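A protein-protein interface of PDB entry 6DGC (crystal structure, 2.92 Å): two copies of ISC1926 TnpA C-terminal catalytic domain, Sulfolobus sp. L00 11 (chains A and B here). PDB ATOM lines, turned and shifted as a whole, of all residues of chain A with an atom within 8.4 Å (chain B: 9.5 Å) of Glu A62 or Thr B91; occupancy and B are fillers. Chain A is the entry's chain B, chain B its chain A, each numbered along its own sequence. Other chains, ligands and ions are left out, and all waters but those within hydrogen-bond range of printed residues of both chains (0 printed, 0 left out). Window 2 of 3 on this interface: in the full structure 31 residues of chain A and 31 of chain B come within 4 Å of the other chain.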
ATOM      1  N   LEU A  54      -7.995  28.967 -33.377  1.00  0.00           N
ATOM      2  CA  LEU A  54      -6.950  28.094 -32.840  1.00  0.00           C
ATOM      3  C   LEU A  54      -7.577  26.992 -31.982  1.00  0.00           C
ATOM      4  O   LEU A  54      -7.225  25.810 -32.139  1.00  0.00           O
ATOM      5  CB  LEU A  54      -5.942  28.912 -32.024  1.00  0.00           C
ATOM      6  CG  LEU A  54      -4.719  28.164 -31.514  1.00  0.00           C
ATOM      7  CD1 LEU A  54      -3.733  27.906 -32.634  1.00  0.00           C
ATOM      8  CD2 LEU A  54      -4.040  28.936 -30.396  1.00  0.00           C
ATOM      9  N   LEU A  55      -8.542  27.364 -31.118  1.00  0.00           N
ATOM     10  CA  LEU A  55      -9.192  26.380 -30.252  1.00  0.00           C
ATOM     11  C   LEU A  55     -10.107  25.396 -31.060  1.00  0.00           C
ATOM     12  O   LEU A  55     -10.284  24.248 -30.636  1.00  0.00           O
ATOM     13  CB  LEU A  55      -9.909  27.053 -29.078  1.00  0.00           C
ATOM     14  CG  LEU A  55      -8.983  27.803 -28.125  1.00  0.00           C
ATOM     15  CD1 LEU A  55      -9.767  28.600 -27.120  1.00  0.00           C
ATOM     16  N   LYS A  56     -10.611  25.829 -32.248  1.00  0.00           N
ATOM     17  CA  LYS A  56     -11.392  24.991 -33.159  1.00  0.00           C
ATOM     18  C   LYS A  56     -10.418  24.032 -33.857  1.00  0.00           C
ATOM     19  O   LYS A  56     -10.767  22.868 -34.080  1.00  0.00           O
ATOM     20  CB  LYS A  56     -12.161  25.837 -34.185  1.00  0.00           C
ATOM     21  CG  LYS A  56     -13.406  26.512 -33.606  1.00  0.00           C
ATOM     22  CD  LYS A  56     -14.262  27.167 -34.697  1.00  0.00           C
ATOM     23  CE  LYS A  56     -15.263  28.176 -34.174  1.00  0.00           C
ATOM     24  NZ  LYS A  56     -14.710  29.567 -34.155  1.00  0.00           N
ATOM     25  N   LEU A  57      -9.174  24.516 -34.141  1.00  0.00           N
ATOM     26  CA  LEU A  57      -8.075  23.744 -34.735  1.00  0.00           C
ATOM     27  C   LEU A  57      -7.635  22.654 -33.769  1.00  0.00           C
ATOM     28  O   LEU A  57      -7.443  21.505 -34.189  1.00  0.00           O
ATOM     29  CB  LEU A  57      -6.898  24.666 -35.103  1.00  0.00           C
ATOM     30  CG  LEU A  57      -5.553  24.023 -35.450  1.00  0.00           C
ATOM     31  CD1 LEU A  57      -5.589  23.337 -36.797  1.00  0.00           C
ATOM     32  CD2 LEU A  57      -4.449  25.060 -35.437  1.00  0.00           C
ATOM     33  N   PHE A  58      -7.510  23.008 -32.473  1.00  0.00           N
ATOM     34  CA  PHE A  58      -7.145  22.051 -31.423  1.00  0.00           C
ATOM     35  C   PHE A  58      -8.151  20.904 -31.369  1.00  0.00           C
ATOM     36  O   PHE A  58      -7.749  19.748 -31.406  1.00  0.00           O
ATOM     37  CB  PHE A  58      -7.046  22.741 -30.058  1.00  0.00           C
ATOM     38  CG  PHE A  58      -5.780  23.532 -29.784  1.00  0.00           C
ATOM     39  CD1 PHE A  58      -4.870  23.813 -30.809  1.00  0.00           C
ATOM     40  CD2 PHE A  58      -5.523  24.042 -28.514  1.00  0.00           C
ATOM     41  CE1 PHE A  58      -3.723  24.563 -30.558  1.00  0.00           C
ATOM     42  CE2 PHE A  58      -4.372  24.791 -28.263  1.00  0.00           C
ATOM     43  CZ  PHE A  58      -3.480  25.044 -29.282  1.00  0.00           C
ATOM     44  N   LYS A  59      -9.456  21.223 -31.379  1.00  0.00           N
ATOM     45  CA  LYS A  59     -10.523  20.232 -31.347  1.00  0.00           C
ATOM     46  C   LYS A  59     -10.554  19.361 -32.609  1.00  0.00           C
ATOM     47  O   LYS A  59     -10.829  18.156 -32.503  1.00  0.00           O
ATOM     48  CB  LYS A  59     -11.880  20.888 -31.063  1.00  0.00           C
ATOM     49  N   LEU A  60     -10.238  19.958 -33.788  1.00  0.00           N
ATOM     50  CA  LEU A  60     -10.204  19.253 -35.073  1.00  0.00           C
ATOM     51  C   LEU A  60      -9.103  18.202 -35.055  1.00  0.00           C
ATOM     52  O   LEU A  60      -9.339  17.033 -35.411  1.00  0.00           O
ATOM     53  CB  LEU A  60      -9.934  20.239 -36.213  1.00  0.00           C
ATOM     54  CG  LEU A  60     -10.664  19.990 -37.548  1.00  0.00           C
ATOM     55  CD1 LEU A  60     -10.611  21.215 -38.413  1.00  0.00           C
ATOM     56  CD2 LEU A  60     -10.074  18.830 -38.342  1.00  0.00           C
ATOM     57  N   VAL A  61      -7.907  18.636 -34.615  1.00  0.00           N
ATOM     58  CA  VAL A  61      -6.735  17.788 -34.519  1.00  0.00           C
ATOM     59  C   VAL A  61      -7.000  16.628 -33.583  1.00  0.00           C
ATOM     60  O   VAL A  61      -6.868  15.476 -34.015  1.00  0.00           O
ATOM     61  CB  VAL A  61      -5.481  18.605 -34.179  1.00  0.00           C
ATOM     62  CG1 VAL A  61      -4.333  17.712 -33.723  1.00  0.00           C
ATOM     63  CG2 VAL A  61      -5.067  19.428 -35.391  1.00  0.00           C
ATOM     64  N   GLU A  62      -7.501  16.933 -32.360  1.00  0.00           N
ATOM     65  CA  GLU A  62      -7.869  15.970 -31.307  1.00  0.00           C
ATOM     66  C   GLU A  62      -8.919  14.921 -31.762  1.00  0.00           C
ATOM     67  O   GLU A  62      -8.905  13.782 -31.284  1.00  0.00           O
ATOM     68  CB  GLU A  62      -8.355  16.709 -30.055  1.00  0.00           C
ATOM     69  CG  GLU A  62      -7.221  17.314 -29.261  1.00  0.00           C
ATOM     70  CD  GLU A  62      -7.578  18.446 -28.317  1.00  0.00           C
ATOM     71  OE1 GLU A  62      -8.668  18.413 -27.696  1.00  0.00           O
ATOM     72  OE2 GLU A  62      -6.716  19.336 -28.141  1.00  0.00           O
ATOM     73  N   GLY A  63      -9.793  15.323 -32.687  1.00  0.00           N
ATOM     74  CA  GLY A  63     -10.822  14.464 -33.257  1.00  0.00           C
ATOM     75  C   GLY A  63     -10.301  13.520 -34.326  1.00  0.00           C
ATOM     76  O   GLY A  63     -11.084  12.780 -34.928  1.00  0.00           O
ATOM     77  N   ARG A  64      -8.962  13.559 -34.583  1.00  0.00           N
ATOM     78  CA  ARG A  64      -8.215  12.729 -35.547  1.00  0.00           C
ATOM     79  C   ARG A  64      -8.828  12.733 -36.970  1.00  0.00           C
ATOM     80  O   ARG A  64      -8.658  11.782 -37.742  1.00  0.00           O
ATOM     81  CB  ARG A  64      -8.006  11.298 -34.999  1.00  0.00           C
ATOM     82  CG  ARG A  64      -6.862  11.225 -33.982  1.00  0.00           C
ATOM     83  CD  ARG A  64      -6.679   9.850 -33.366  1.00  0.00           C
ATOM     84  NE  ARG A  64      -5.410   9.745 -32.637  1.00  0.00           N
ATOM     85  CZ  ARG A  64      -5.234  10.090 -31.361  1.00  0.00           C
ATOM     86  NH1 ARG A  64      -4.045   9.948 -30.786  1.00  0.00           N
ATOM     87  NH2 ARG A  64      -6.245  10.579 -30.650  1.00  0.00           N
ATOM     88  N   SER A  65      -9.496  13.843 -37.314  1.00  0.00           N
ATOM     89  CA  SER A  65     -10.142  14.067 -38.604  1.00  0.00           C
ATOM     90  C   SER A  65      -9.087  14.416 -39.674  1.00  0.00           C
ATOM     91  O   SER A  65      -9.062  13.816 -40.751  1.00  0.00           O
ATOM     92  CB  SER A  65     -11.181  15.181 -38.467  1.00  0.00           C
ATOM     93  OG  SER A  65     -11.755  15.530 -39.714  1.00  0.00           O
ATOM     94  N   VAL A  66      -8.202  15.362 -39.337  1.00  0.00           N
ATOM     95  CA  VAL A  66      -7.124  15.874 -40.176  1.00  0.00           C
ATOM     96  C   VAL A  66      -5.780  15.125 -39.960  1.00  0.00           C
ATOM     97  O   VAL A  66      -5.559  14.557 -38.881  1.00  0.00           O
ATOM     98  CB  VAL A  66      -7.008  17.409 -39.965  1.00  0.00           C
ATOM     99  CG1 VAL A  66      -6.382  17.774 -38.617  1.00  0.00           C
ATOM    100  CG2 VAL A  66      -6.267  18.060 -41.110  1.00  0.00           C
ATOM    101  N   GLU A  87       3.852  19.463 -29.985  1.00  0.00           N
ATOM    102  CA  GLU A  87       3.752  18.251 -29.166  1.00  0.00           C
ATOM    103  C   GLU A  87       2.298  17.742 -29.038  1.00  0.00           C
ATOM    104  O   GLU A  87       2.058  16.537 -29.114  1.00  0.00           O
ATOM    105  CB  GLU A  87       4.419  18.461 -27.801  1.00  0.00           C
ATOM    106  CG  GLU A  87       4.598  17.193 -26.984  1.00  0.00           C
ATOM    107  CD  GLU A  87       5.747  16.291 -27.387  1.00  0.00           C
ATOM    108  OE1 GLU A  87       6.894  16.575 -26.973  1.00  0.00           O
ATOM    109  OE2 GLU A  87       5.497  15.271 -28.070  1.00  0.00           O
ATOM    110  N   LEU A  88       1.335  18.660 -28.863  1.00  0.00           N
ATOM    111  CA  LEU A  88      -0.089  18.312 -28.741  1.00  0.00           C
ATOM    112  C   LEU A  88      -0.573  17.620 -30.019  1.00  0.00           C
ATOM    113  O   LEU A  88      -1.209  16.565 -29.942  1.00  0.00           O
ATOM    114  CB  LEU A  88      -0.923  19.586 -28.427  1.00  0.00           C
ATOM    115  CG  LEU A  88      -2.430  19.527 -28.658  1.00  0.00           C
ATOM    116  CD1 LEU A  88      -3.134  18.636 -27.635  1.00  0.00           C
ATOM    117  CD2 LEU A  88      -3.013  20.910 -28.673  1.00  0.00           C
ATOM    118  N   PHE A  89      -0.225  18.217 -31.185  1.00  0.00           N
ATOM    119  CA  PHE A  89      -0.583  17.742 -32.512  1.00  0.00           C
ATOM    120  C   PHE A  89       0.068  16.413 -32.821  1.00  0.00           C
ATOM    121  O   PHE A  89      -0.634  15.482 -33.187  1.00  0.00           O
ATOM    122  CB  PHE A  89      -0.239  18.788 -33.571  1.00  0.00           C
ATOM    123  CG  PHE A  89      -1.114  20.024 -33.579  1.00  0.00           C
ATOM    124  CD1 PHE A  89      -2.020  20.269 -32.545  1.00  0.00           C
ATOM    125  CD2 PHE A  89      -1.016  20.963 -34.610  1.00  0.00           C
ATOM    126  CE1 PHE A  89      -2.813  21.420 -32.546  1.00  0.00           C
ATOM    127  CE2 PHE A  89      -1.812  22.113 -34.608  1.00  0.00           C
ATOM    128  CZ  PHE A  89      -2.714  22.327 -33.583  1.00  0.00           C
ATOM    129  N   THR A  91       1.049  14.016 -30.906  1.00  0.00           N
ATOM    130  CA  THR A  91       0.463  12.897 -30.153  1.00  0.00           C
ATOM    131  C   THR A  91      -0.803  12.381 -30.868  1.00  0.00           C
ATOM    132  O   THR A  91      -1.135  11.207 -30.749  1.00  0.00           O
ATOM    133  CB  THR A  91       0.271  13.236 -28.660  1.00  0.00           C
ATOM    134  OG1 THR A  91      -0.774  14.195 -28.511  1.00  0.00           O
ATOM    135  N   MET A  92      -1.445  13.248 -31.681  1.00  0.00           N
ATOM    136  CA  MET A  92      -2.625  12.916 -32.501  1.00  0.00           C
ATOM    137  C   MET A  92      -2.175  12.482 -33.916  1.00  0.00           C
ATOM    138  O   MET A  92      -3.022  12.211 -34.781  1.00  0.00           O
ATOM    139  CB  MET A  92      -3.601  14.117 -32.597  1.00  0.00           C
ATOM    140  CG  MET A  92      -3.991  14.721 -31.272  1.00  0.00           C
ATOM    141  SD  MET A  92      -4.890  13.569 -30.214  1.00  0.00           S
ATOM    142  N   GLY A  93      -0.852  12.424 -34.130  1.00  0.00           N
ATOM    143  CA  GLY A  93      -0.236  12.044 -35.402  1.00  0.00           C
ATOM    144  C   GLY A  93      -0.446  13.058 -36.505  1.00  0.00           C
ATOM    145  O   GLY A  93      -0.572  12.705 -37.679  1.00  0.00           O
ATOM    146  N   VAL A  94      -0.513  14.326 -36.125  1.00  0.00           N
ATOM    147  CA  VAL A  94      -0.720  15.445 -37.030  1.00  0.00           C
ATOM    148  C   VAL A  94       0.604  16.198 -37.115  1.00  0.00           C
ATOM    149  O   VAL A  94       1.213  16.511 -36.068  1.00  0.00           O
ATOM    150  CB  VAL A  94      -1.905  16.333 -36.554  1.00  0.00           C
ATOM    151  CG1 VAL A  94      -1.963  17.659 -37.302  1.00  0.00           C
ATOM    152  CG2 VAL A  94      -3.231  15.588 -36.679  1.00  0.00           C
ATOM    153  N   PHE B  58       6.515  15.553 -20.131  1.00  0.00           N
ATOM    154  CA  PHE B  58       5.676  15.394 -21.314  1.00  0.00           C
ATOM    155  C   PHE B  58       5.554  13.910 -21.657  1.00  0.00           C
ATOM    156  O   PHE B  58       4.433  13.419 -21.805  1.00  0.00           O
ATOM    157  CB  PHE B  58       6.237  16.186 -22.497  1.00  0.00           C
ATOM    158  CG  PHE B  58       5.956  17.667 -22.515  1.00  0.00           C
ATOM    159  CD1 PHE B  58       5.422  18.309 -21.403  1.00  0.00           C
ATOM    160  CD2 PHE B  58       6.265  18.435 -23.633  1.00  0.00           C
ATOM    161  CE1 PHE B  58       5.180  19.691 -21.423  1.00  0.00           C
ATOM    162  CE2 PHE B  58       6.034  19.815 -23.648  1.00  0.00           C
ATOM    163  CZ  PHE B  58       5.479  20.433 -22.551  1.00  0.00           C
ATOM    164  N   VAL B  61       3.397  11.922 -18.873  1.00  0.00           N
ATOM    165  CA  VAL B  61       1.975  12.221 -19.068  1.00  0.00           C
ATOM    166  C   VAL B  61       1.441  11.489 -20.305  1.00  0.00           C
ATOM    167  O   VAL B  61       0.388  10.863 -20.213  1.00  0.00           O
ATOM    168  CB  VAL B  61       1.736  13.745 -19.143  1.00  0.00           C
ATOM    169  CG1 VAL B  61       0.334  14.066 -19.627  1.00  0.00           C
ATOM    170  CG2 VAL B  61       1.993  14.396 -17.799  1.00  0.00           C
ATOM    171  N   GLU B  62       2.183  11.539 -21.438  1.00  0.00           N
ATOM    172  CA  GLU B  62       1.846  10.851 -22.697  1.00  0.00           C
ATOM    173  C   GLU B  62       1.779   9.297 -22.556  1.00  0.00           C
ATOM    174  O   GLU B  62       1.010   8.639 -23.265  1.00  0.00           O
ATOM    175  CB  GLU B  62       2.824  11.251 -23.813  1.00  0.00           C
ATOM    176  CG  GLU B  62       2.546  12.631 -24.367  1.00  0.00           C
ATOM    177  CD  GLU B  62       3.687  13.305 -25.103  1.00  0.00           C
ATOM    178  OE1 GLU B  62       4.477  12.609 -25.786  1.00  0.00           O
ATOM    179  OE2 GLU B  62       3.753  14.554 -25.040  1.00  0.00           O
ATOM    180  N   ARG B  64       0.557   7.838 -20.061  1.00  0.00           N
ATOM    181  CA  ARG B  64      -0.645   7.659 -19.229  1.00  0.00           C
ATOM    182  C   ARG B  64      -0.355   6.971 -17.880  1.00  0.00           C
ATOM    183  O   ARG B  64      -1.243   6.347 -17.290  1.00  0.00           O
ATOM    184  CB  ARG B  64      -1.763   6.943 -20.022  1.00  0.00           C
ATOM    185  N   GLU B  83      -1.545  27.313 -21.395  1.00  0.00           N
ATOM    186  CA  GLU B  83      -2.811  26.836 -21.950  1.00  0.00           C
ATOM    187  C   GLU B  83      -2.626  25.699 -22.930  1.00  0.00           C
ATOM    188  O   GLU B  83      -3.466  24.789 -22.956  1.00  0.00           O
ATOM    189  CB  GLU B  83      -3.617  28.014 -22.552  1.00  0.00           C
ATOM    190  CG  GLU B  83      -3.957  29.139 -21.559  1.00  0.00           C
ATOM    191  CD  GLU B  83      -4.719  28.691 -20.317  1.00  0.00           C
ATOM    192  OE1 GLU B  83      -5.813  28.096 -20.469  1.00  0.00           O
ATOM    193  OE2 GLU B  83      -4.202  28.897 -19.193  1.00  0.00           O
ATOM    194  N   TYR B  84      -1.498  25.720 -23.695  1.00  0.00           N
ATOM    195  CA  TYR B  84      -1.148  24.665 -24.661  1.00  0.00           C
ATOM    196  C   TYR B  84      -0.733  23.406 -23.899  1.00  0.00           C
ATOM    197  O   TYR B  84      -1.176  22.308 -24.246  1.00  0.00           O
ATOM    198  CB  TYR B  84      -0.021  25.105 -25.616  1.00  0.00           C
ATOM    199  CG  TYR B  84      -0.236  26.433 -26.318  1.00  0.00           C
ATOM    200  CD1 TYR B  84      -1.470  26.765 -26.870  1.00  0.00           C
ATOM    201  CD2 TYR B  84       0.823  27.314 -26.526  1.00  0.00           C
ATOM    202  CE1 TYR B  84      -1.664  27.974 -27.543  1.00  0.00           C
ATOM    203  CE2 TYR B  84       0.640  28.527 -27.198  1.00  0.00           C
ATOM    204  CZ  TYR B  84      -0.607  28.854 -27.706  1.00  0.00           C
ATOM    205  OH  TYR B  84      -0.821  30.061 -28.340  1.00  0.00           O
ATOM    206  N   ILE B  85       0.087  23.575 -22.827  1.00  0.00           N
ATOM    207  CA  ILE B  85       0.542  22.452 -21.987  1.00  0.00           C
ATOM    208  C   ILE B  85      -0.671  21.834 -21.311  1.00  0.00           C
ATOM    209  O   ILE B  85      -0.817  20.612 -21.339  1.00  0.00           O
ATOM    210  CB  ILE B  85       1.675  22.799 -20.998  1.00  0.00           C
ATOM    211  CG1 ILE B  85       2.855  23.456 -21.704  1.00  0.00           C
ATOM    212  CG2 ILE B  85       2.134  21.540 -20.284  1.00  0.00           C
ATOM    213  CD1 ILE B  85       4.022  23.786 -20.815  1.00  0.00           C
ATOM    214  N   GLU B  86      -1.576  22.694 -20.785  1.00  0.00           N
ATOM    215  CA  GLU B  86      -2.835  22.319 -20.139  1.00  0.00           C
ATOM    216  C   GLU B  86      -3.658  21.462 -21.092  1.00  0.00           C
ATOM    217  O   GLU B  86      -4.190  20.433 -20.676  1.00  0.00           O
ATOM    218  CB  GLU B  86      -3.638  23.567 -19.757  1.00  0.00           C
ATOM    219  CG  GLU B  86      -4.257  23.510 -18.377  1.00  0.00           C
ATOM    220  CD  GLU B  86      -5.321  24.568 -18.142  1.00  0.00           C
ATOM    221  OE1 GLU B  86      -4.965  25.736 -17.856  1.00  0.00           O
ATOM    222  OE2 GLU B  86      -6.519  24.230 -18.276  1.00  0.00           O
ATOM    223  N   GLU B  87      -3.700  21.848 -22.378  1.00  0.00           N
ATOM    224  CA  GLU B  87      -4.440  21.118 -23.407  1.00  0.00           C
ATOM    225  C   GLU B  87      -3.783  19.764 -23.744  1.00  0.00           C
ATOM    226  O   GLU B  87      -4.494  18.778 -23.936  1.00  0.00           O
ATOM    227  CB  GLU B  87      -4.633  21.981 -24.662  1.00  0.00           C
ATOM    228  CG  GLU B  87      -5.601  21.382 -25.670  1.00  0.00           C
ATOM    229  CD  GLU B  87      -7.087  21.438 -25.356  1.00  0.00           C
ATOM    230  OE1 GLU B  87      -7.778  20.425 -25.619  1.00  0.00           O
ATOM    231  OE2 GLU B  87      -7.565  22.491 -24.873  1.00  0.00           O
ATOM    232  N   LEU B  88      -2.434  19.721 -23.806  1.00  0.00           N
ATOM    233  CA  LEU B  88      -1.683  18.502 -24.120  1.00  0.00           C
ATOM    234  C   LEU B  88      -1.939  17.463 -23.039  1.00  0.00           C
ATOM    235  O   LEU B  88      -2.235  16.311 -23.360  1.00  0.00           O
ATOM    236  CB  LEU B  88      -0.175  18.822 -24.274  1.00  0.00           C
ATOM    237  CG  LEU B  88       0.829  17.664 -24.176  1.00  0.00           C
ATOM    238  CD1 LEU B  88       0.764  16.752 -25.382  1.00  0.00           C
ATOM    239  CD2 LEU B  88       2.245  18.180 -23.965  1.00  0.00           C
ATOM    240  N   PHE B  89      -1.869  17.894 -21.762  1.00  0.00           N
ATOM    241  CA  PHE B  89      -2.078  17.068 -20.574  1.00  0.00           C
ATOM    242  C   PHE B  89      -3.501  16.573 -20.471  1.00  0.00           C
ATOM    243  O   PHE B  89      -3.707  15.370 -20.368  1.00  0.00           O
ATOM    244  CB  PHE B  89      -1.655  17.813 -19.312  1.00  0.00           C
ATOM    245  CG  PHE B  89      -0.159  17.986 -19.147  1.00  0.00           C
ATOM    246  CD1 PHE B  89       0.724  17.683 -20.187  1.00  0.00           C
ATOM    247  CD2 PHE B  89       0.370  18.469 -17.961  1.00  0.00           C
ATOM    248  CE1 PHE B  89       2.103  17.861 -20.039  1.00  0.00           C
ATOM    249  CE2 PHE B  89       1.749  18.652 -17.813  1.00  0.00           C
ATOM    250  CZ  PHE B  89       2.606  18.337 -18.850  1.00  0.00           C
ATOM    251  N   SER B  90      -4.485  17.473 -20.585  1.00  0.00           N
ATOM    252  CA  SER B  90      -5.901  17.122 -20.530  1.00  0.00           C
ATOM    253  C   SER B  90      -6.310  16.044 -21.525  1.00  0.00           C
ATOM    254  O   SER B  90      -7.163  15.241 -21.192  1.00  0.00           O
ATOM    255  CB  SER B  90      -6.761  18.355 -20.727  1.00  0.00           C
ATOM    256  OG  SER B  90      -6.506  18.868 -22.025  1.00  0.00           O
ATOM    257  N   THR B  91      -5.710  16.011 -22.733  1.00  0.00           N
ATOM    258  CA  THR B  91      -6.037  14.981 -23.739  1.00  0.00           C
ATOM    259  C   THR B  91      -5.563  13.612 -23.270  1.00  0.00           C
ATOM    260  O   THR B  91      -6.141  12.597 -23.684  1.00  0.00           O
ATOM    261  CB  THR B  91      -5.562  15.327 -25.155  1.00  0.00           C
ATOM    262  OG1 THR B  91      -4.139  15.334 -25.211  1.00  0.00           O
ATOM    263  CG2 THR B  91      -6.165  16.595 -25.687  1.00  0.00           C
ATOM    264  N   MET B  92      -4.554  13.594 -22.359  1.00  0.00           N
ATOM    265  CA  MET B  92      -4.034  12.376 -21.729  1.00  0.00           C
ATOM    266  C   MET B  92      -4.778  12.113 -20.392  1.00  0.00           C
ATOM    267  O   MET B  92      -4.433  11.177 -19.673  1.00  0.00           O
ATOM    268  CB  MET B  92      -2.516  12.468 -21.485  1.00  0.00           C
ATOM    269  CG  MET B  92      -1.707  12.862 -22.709  1.00  0.00           C
ATOM    270  SD  MET B  92      -1.805  11.713 -24.110  1.00  0.00           S
ATOM    271  N   GLY B  93      -5.784  12.944 -20.088  1.00  0.00           N
ATOM    272  CA  GLY B  93      -6.594  12.856 -18.873  1.00  0.00           C
ATOM    273  C   GLY B  93      -5.822  13.193 -17.612  1.00  0.00           C
ATOM    274  O   GLY B  93      -6.103  12.650 -16.543  1.00  0.00           O
ATOM    275  N   VAL B  94      -4.831  14.084 -17.736  1.00  0.00           N
ATOM    276  CA  VAL B  94      -3.971  14.525 -16.650  1.00  0.00           C
ATOM    277  C   VAL B  94      -4.358  15.954 -16.310  1.00  0.00           C
ATOM    278  O   VAL B  94      -4.490  16.787 -17.209  1.00  0.00           O
ATOM    279  CB  VAL B  94      -2.471  14.364 -17.031  1.00  0.00           C
ATOM    280  CG1 VAL B  94      -1.552  15.067 -16.046  1.00  0.00           C
ATOM    281  CG2 VAL B  94      -2.089  12.893 -17.159  1.00  0.00           C
ATOM    282  N   LYS B  95      -4.575  16.221 -15.016  1.00  0.00           N
ATOM    283  CA  LYS B  95      -4.938  17.536 -14.494  1.00  0.00           C
ATOM    284  C   LYS B  95      -3.692  18.206 -13.946  1.00  0.00           C
ATOM    285  O   LYS B  95      -2.826  17.516 -13.422  1.00  0.00           O
ATOM    286  CB  LYS B  95      -6.001  17.398 -13.370  1.00  0.00           C
ATOM    287  CG  LYS B  95      -6.036  18.553 -12.352  1.00  0.00           C
ATOM    288  CD  LYS B  95      -7.070  18.361 -11.271  1.00  0.00           C
ATOM    289  CE  LYS B  95      -7.397  19.646 -10.550  1.00  0.00           C
ATOM    290  NZ  LYS B  95      -8.376  19.424  -9.451  1.00  0.00           N
ATOM    291  N   ILE B  96      -3.600  19.545 -14.057  1.00  0.00           N
ATOM    292  CA  ILE B  96      -2.518  20.318 -13.442  1.00  0.00           C
ATOM    293  C   ILE B  96      -3.111  20.965 -12.174  1.00  0.00           C
ATOM    294  O   ILE B  96      -4.071  21.740 -12.266  1.00  0.00           O
ATOM    295  CB  ILE B  96      -1.872  21.372 -14.379  1.00  0.00           C
ATOM    296  CG1 ILE B  96      -1.326  20.718 -15.659  1.00  0.00           C
ATOM    297  CG2 ILE B  96      -0.760  22.136 -13.633  1.00  0.00           C
ATOM    298  CD1 ILE B  96      -1.045  21.676 -16.783  1.00  0.00           C
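The side-chain carboxylate of Glu B87 sits close to the side-chain carboxylate of Glu A62 (2.9 Å).
The backbone carbonyl oxygen (O) of Glu B87 sits at hydrogen-bond distance from the side-chain hydroxyl (OG) of Ser B90. The backbone carbonyl oxygen (O) of Leu B88 lies within hydrogen-bond range of the side-chain hydroxyl (OG1) of Thr B91, 2.8 Å away. O of Leu A88 sits at hydrogen-bond distance from OG1 of Thr A91 (2.8 Å).
Tyr B84 touches Leu A54 (CE1 to CD2, 3.8 Å). CD1 of Tyr B84 touches CZ of Phe A58, at 3.6 Å. CG of Glu B87 touches CD2 of Phe A58 (3.9 Å). Thr B91 touches Glu A62. Glu A87 touches Phe B58 (OE1 to CD2, 3.9 Å). Glu B62 touches Glu A87 (OE2 to CG, 3.4 Å). CD2 of Leu B88 touches CG of Glu A87 (3.95 Å). Glu B87 touches Leu A88. CA of Leu A88 touches CD1 of Leu B88, 3.8 Å away.
No residue of chain B comes within 4 Å of Val A61. Glu A62 touches two residues of chain B. Printed residues of chain A within 4 Å of Tyr B84: Leu A54 (3.8 Å) and Phe A58 (3.6 Å). Printed residues of chain A within 4 Å of Leu B88: Glu A87 and Leu A88. No residue of chain A comes within 4 Å of Ser B90. Thr B91 touches just one residue of chain A: Glu A62 (3.5 Å). The nearest printed residue of chain A that does not touch Tyr B84 is Leu A88 (5.0 Å).
Along chain B the printed residues that touch a printed residue of chain A span positions 58 to 91. Hydrophobic or aromatic side chains of chain A that line the printed part of chain B: Leu A54, Phe A58 and Leu A88. Among the printed residues, 10 pairs touch across the chains.
Phe A58 touches Glu B87, and with the chains exchanged Glu A87 touches Phe B58. Glu A62 touches Glu B87, and with the chains exchanged Glu A87 touches Glu B62. Glu A62 touches Thr B91, but with the chains exchanged Thr A91 does not touch Glu B62 (4.9 Å). Leu B88 touches its own counterpart, Leu A88. Of the 10 pairs that touch across the chains among the printed residues, 7 have their exchanged pair printed and touching as well.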
